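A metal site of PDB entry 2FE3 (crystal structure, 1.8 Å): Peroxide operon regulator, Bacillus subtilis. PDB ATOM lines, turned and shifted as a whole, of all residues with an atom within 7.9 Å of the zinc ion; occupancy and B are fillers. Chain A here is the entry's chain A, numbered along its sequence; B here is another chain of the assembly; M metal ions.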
ATOM      1  N   ILE A  95     -27.521  16.573  17.786  1.00  0.00           N
ATOM      2  CA  ILE A  95     -28.581  15.584  17.974  1.00  0.00           C
ATOM      3  C   ILE A  95     -29.279  15.332  16.637  1.00  0.00           C
ATOM      4  O   ILE A  95     -29.802  16.276  16.032  1.00  0.00           O
ATOM      5  CB  ILE A  95     -29.619  16.024  19.038  1.00  0.00           C
ATOM      6  CG1 ILE A  95     -28.913  16.226  20.404  1.00  0.00           C
ATOM      7  CG2 ILE A  95     -30.751  14.986  19.158  1.00  0.00           C
ATOM      8  CD1 ILE A  95     -29.786  16.817  21.453  1.00  0.00           C
ATOM      9  N   CYS A  96     -29.252  14.083  16.175  1.00  0.00           N
ATOM     10  CA  CYS A  96     -29.907  13.749  14.886  1.00  0.00           C
ATOM     11  C   CYS A  96     -31.413  13.588  15.044  1.00  0.00           C
ATOM     12  O   CYS A  96     -31.885  12.711  15.801  1.00  0.00           O
ATOM     13  CB  CYS A  96     -29.325  12.461  14.275  1.00  0.00           C
ATOM     14  SG  CYS A  96     -30.062  12.161  12.617  1.00  0.00           S
ATOM     15  N   GLU A  97     -32.163  14.392  14.276  1.00  0.00           N
ATOM     16  CA  GLU A  97     -33.627  14.385  14.310  1.00  0.00           C
ATOM     17  C   GLU A  97     -34.220  13.115  13.666  1.00  0.00           C
ATOM     18  O   GLU A  97     -35.376  12.777  13.903  1.00  0.00           O
ATOM     19  CB  GLU A  97     -34.192  15.653  13.648  1.00  0.00           C
ATOM     20  CG  GLU A  97     -33.639  16.954  14.258  1.00  0.00           C
ATOM     21  CD  GLU A  97     -34.537  18.147  14.015  1.00  0.00           C
ATOM     22  OE1 GLU A  97     -34.229  18.937  13.081  1.00  0.00           O
ATOM     23  OE2 GLU A  97     -35.533  18.290  14.753  1.00  0.00           O
ATOM     24  N   ASN A  98     -33.415  12.416  12.879  1.00  0.00           N
ATOM     25  CA  ASN A  98     -33.905  11.238  12.148  1.00  0.00           C
ATOM     26  C   ASN A  98     -33.642   9.911  12.850  1.00  0.00           C
ATOM     27  O   ASN A  98     -34.504   9.044  12.848  1.00  0.00           O
ATOM     28  CB  ASN A  98     -33.296  11.201  10.745  1.00  0.00           C
ATOM     29  CG  ASN A  98     -33.751  12.365   9.867  1.00  0.00           C
ATOM     30  OD1 ASN A  98     -34.430  13.303  10.328  1.00  0.00           O
ATOM     31  ND2 ASN A  98     -33.361  12.322   8.597  1.00  0.00           N
ATOM     32  N   CYS A  99     -32.466   9.755  13.456  1.00  0.00           N
ATOM     33  CA  CYS A  99     -32.113   8.481  14.060  1.00  0.00           C
ATOM     34  C   CYS A  99     -31.890   8.624  15.565  1.00  0.00           C
ATOM     35  O   CYS A  99     -31.773   7.625  16.233  1.00  0.00           O
ATOM     36  CB  CYS A  99     -30.863   7.864  13.392  1.00  0.00           C
ATOM     37  SG  CYS A  99     -29.262   8.655  13.796  1.00  0.00           S
ATOM     38  N   GLY A 100     -31.858   9.853  16.082  1.00  0.00           N
ATOM     39  CA  GLY A 100     -31.687  10.098  17.507  1.00  0.00           C
ATOM     40  C   GLY A 100     -30.247  10.032  18.016  1.00  0.00           C
ATOM     41  O   GLY A 100     -30.010  10.144  19.211  1.00  0.00           O
ATOM     42  N   LYS A 101     -29.282   9.888  17.103  1.00  0.00           N
ATOM     43  CA  LYS A 101     -27.849   9.880  17.448  1.00  0.00           C
ATOM     44  C   LYS A 101     -27.442  11.186  18.149  1.00  0.00           C
ATOM     45  O   LYS A 101     -27.807  12.252  17.719  1.00  0.00           O
ATOM     46  CB  LYS A 101     -27.026   9.742  16.174  1.00  0.00           C
ATOM     47  CG  LYS A 101     -25.544   9.641  16.410  1.00  0.00           C
ATOM     48  CD  LYS A 101     -24.757   9.547  15.106  1.00  0.00           C
ATOM     49  CE  LYS A 101     -25.141   8.349  14.274  1.00  0.00           C
ATOM     50  NZ  LYS A 101     -24.249   8.272  13.085  1.00  0.00           N
ATOM     51  N   ILE A 102     -26.672  11.081  19.228  1.00  0.00           N
ATOM     52  CA  ILE A 102     -26.128  12.296  19.903  1.00  0.00           C
ATOM     53  C   ILE A 102     -24.590  12.213  19.802  1.00  0.00           C
ATOM     54  O   ILE A 102     -23.976  11.158  20.076  1.00  0.00           O
ATOM     55  CB  ILE A 102     -26.579  12.387  21.367  1.00  0.00           C
ATOM     56  CG1 ILE A 102     -28.100  12.385  21.474  1.00  0.00           C
ATOM     57  CG2 ILE A 102     -25.937  13.606  22.075  1.00  0.00           C
ATOM     58  CD1 ILE A 102     -28.609  12.380  22.908  1.00  0.00           C
ATOM     59  N   GLY A 134     -30.198  18.540  13.971  1.00  0.00           N
ATOM     60  CA  GLY A 134     -30.046  18.448  12.528  1.00  0.00           C
ATOM     61  C   GLY A 134     -30.023  16.995  12.108  1.00  0.00           C
ATOM     62  O   GLY A 134     -30.709  16.162  12.689  1.00  0.00           O
ATOM     63  N   VAL A 135     -29.257  16.708  11.067  1.00  0.00           N
ATOM     64  CA  VAL A 135     -29.221  15.343  10.517  1.00  0.00           C
ATOM     65  C   VAL A 135     -27.776  14.890  10.464  1.00  0.00           C
ATOM     66  O   VAL A 135     -26.923  15.580   9.892  1.00  0.00           O
ATOM     67  CB  VAL A 135     -29.895  15.310   9.117  1.00  0.00           C
ATOM     68  CG1 VAL A 135     -29.748  13.916   8.512  1.00  0.00           C
ATOM     69  CG2 VAL A 135     -31.377  15.661   9.267  1.00  0.00           C
ATOM     70  N   CYS A 136     -27.500  13.717  11.048  1.00  0.00           N
ATOM     71  CA  CYS A 136     -26.157  13.172  11.081  1.00  0.00           C
ATOM     72  C   CYS A 136     -25.652  12.796   9.687  1.00  0.00           C
ATOM     73  O   CYS A 136     -26.431  12.625   8.745  1.00  0.00           O
ATOM     74  CB  CYS A 136     -26.096  11.987  12.050  1.00  0.00           C
ATOM     75  SG  CYS A 136     -26.782  10.444  11.392  1.00  0.00           S
ATOM     76  N   GLN A 137     -24.340  12.619   9.579  1.00  0.00           N
ATOM     77  CA  GLN A 137     -23.710  12.270   8.296  1.00  0.00           C
ATOM     78  C   GLN A 137     -24.311  10.990   7.697  1.00  0.00           C
ATOM     79  O   GLN A 137     -24.551  10.928   6.487  1.00  0.00           O
ATOM     80  CB  GLN A 137     -22.208  12.123   8.482  1.00  0.00           C
ATOM     81  CG  GLN A 137     -21.425  12.380   7.226  1.00  0.00           C
ATOM     82  CD  GLN A 137     -19.941  12.520   7.531  1.00  0.00           C
ATOM     83  OE1 GLN A 137     -19.312  13.516   7.171  1.00  0.00           O
ATOM     84  NE2 GLN A 137     -19.386  11.555   8.250  1.00  0.00           N
ATOM     85  N   GLU A 138     -24.583   9.993   8.530  1.00  0.00           N
ATOM     86  CA  GLU A 138     -25.072   8.695   8.023  1.00  0.00           C
ATOM     87  C   GLU A 138     -26.478   8.839   7.423  1.00  0.00           C
ATOM     88  O   GLU A 138     -26.797   8.276   6.355  1.00  0.00           O
ATOM     89  CB  GLU A 138     -25.085   7.652   9.122  1.00  0.00           C
ATOM     90  CG  GLU A 138     -23.728   7.138   9.561  1.00  0.00           C
ATOM     91  CD  GLU A 138     -23.854   5.879  10.440  1.00  0.00           C
ATOM     92  OE1 GLU A 138     -24.780   5.790  11.286  1.00  0.00           O
ATOM     93  OE2 GLU A 138     -22.993   4.970  10.284  1.00  0.00           O
ATOM     94  N   CYS A 139     -27.317   9.601   8.113  1.00  0.00           N
ATOM     95  CA  CYS A 139     -28.695   9.793   7.689  1.00  0.00           C
ATOM     96  C   CYS A 139     -28.733  10.675   6.459  1.00  0.00           C
ATOM     97  O   CYS A 139     -29.543  10.460   5.570  1.00  0.00           O
ATOM     98  CB  CYS A 139     -29.533  10.396   8.815  1.00  0.00           C
ATOM     99  SG  CYS A 139     -29.959   9.227  10.173  1.00  0.00           S
ATOM    100  N   SER A 140     -27.870  11.682   6.430  1.00  0.00           N
ATOM    101  CA  SER A 140     -27.764  12.576   5.289  1.00  0.00           C
ATOM    102  C   SER A 140     -27.349  11.789   4.027  1.00  0.00           C
ATOM    103  O   SER A 140     -27.916  11.961   2.970  1.00  0.00           O
ATOM    104  CB  SER A 140     -26.756  13.677   5.595  1.00  0.00           C
ATOM    105  OG  SER A 140     -26.685  14.605   4.535  1.00  0.00           O
ATOM    106  N   GLU A 143     -30.306   9.615   2.847  1.00  0.00           N
ATOM    107  CA  GLU A 143     -31.410  10.374   2.289  1.00  0.00           C
ATOM    108  C   GLU A 143     -31.010  11.260   1.108  1.00  0.00           C
ATOM    109  O   GLU A 143     -31.850  12.002   0.573  1.00  0.00           O
ATOM    110  CB  GLU A 143     -32.034  11.253   3.365  1.00  0.00           C
ATOM    111  CG  GLU A 143     -32.650  10.480   4.510  1.00  0.00           C
ATOM    112  CD  GLU A 143     -33.220  11.411   5.584  1.00  0.00           C
ATOM    113  OE1 GLU A 143     -33.022  12.655   5.470  1.00  0.00           O
ATOM    114  OE2 GLU A 143     -33.877  10.909   6.507  1.00  0.00           O
ATOM    115  N   PHE B 123     -22.686  16.847  10.832  1.00  0.00           N
ATOM    116  CA  PHE B 123     -24.133  17.097  10.785  1.00  0.00           C
ATOM    117  C   PHE B 123     -24.500  18.220   9.818  1.00  0.00           C
ATOM    118  O   PHE B 123     -23.732  19.174   9.652  1.00  0.00           O
ATOM    119  CB  PHE B 123     -24.625  17.522  12.157  1.00  0.00           C
ATOM    120  CG  PHE B 123     -24.977  16.397  13.072  1.00  0.00           C
ATOM    121  CD1 PHE B 123     -24.032  15.411  13.370  1.00  0.00           C
ATOM    122  CD2 PHE B 123     -26.223  16.351  13.705  1.00  0.00           C
ATOM    123  CE1 PHE B 123     -24.363  14.370  14.237  1.00  0.00           C
ATOM    124  CE2 PHE B 123     -26.546  15.306  14.577  1.00  0.00           C
ATOM    125  CZ  PHE B 123     -25.625  14.343  14.851  1.00  0.00           C
HETATM  126 ZN    ZN M   1     -28.971  10.149  12.062  1.00  0.00          ZN
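The zinc ion is bound by the side-chain sulfur (SG) of Cys 99, the side-chain sulfur (SG) of Cys 136, the side-chain sulfur (SG) of Cys 139 and the side-chain sulfur (SG) of Cys 96.
N of Cys 96 sits at hydrogen-bond distance from O of Lys 101 (2.8 Å).
The backbone NH (N) of Asn 98 lies close to the side-chain sulfur (SG) of Cys 96 (3.4 Å).
The backbone NH of Lys 101 lies close to the side-chain sulfur of Cys 99 (3.5 Å).
The side-chain sulfur (SG) of Cys 136 lies close to the side-chain amino group (NZ) of Lys 101, 3.7 Å away.
The side-chain sulfur (SG) of Cys 136 sits close to the backbone NH (N) of Glu 138.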
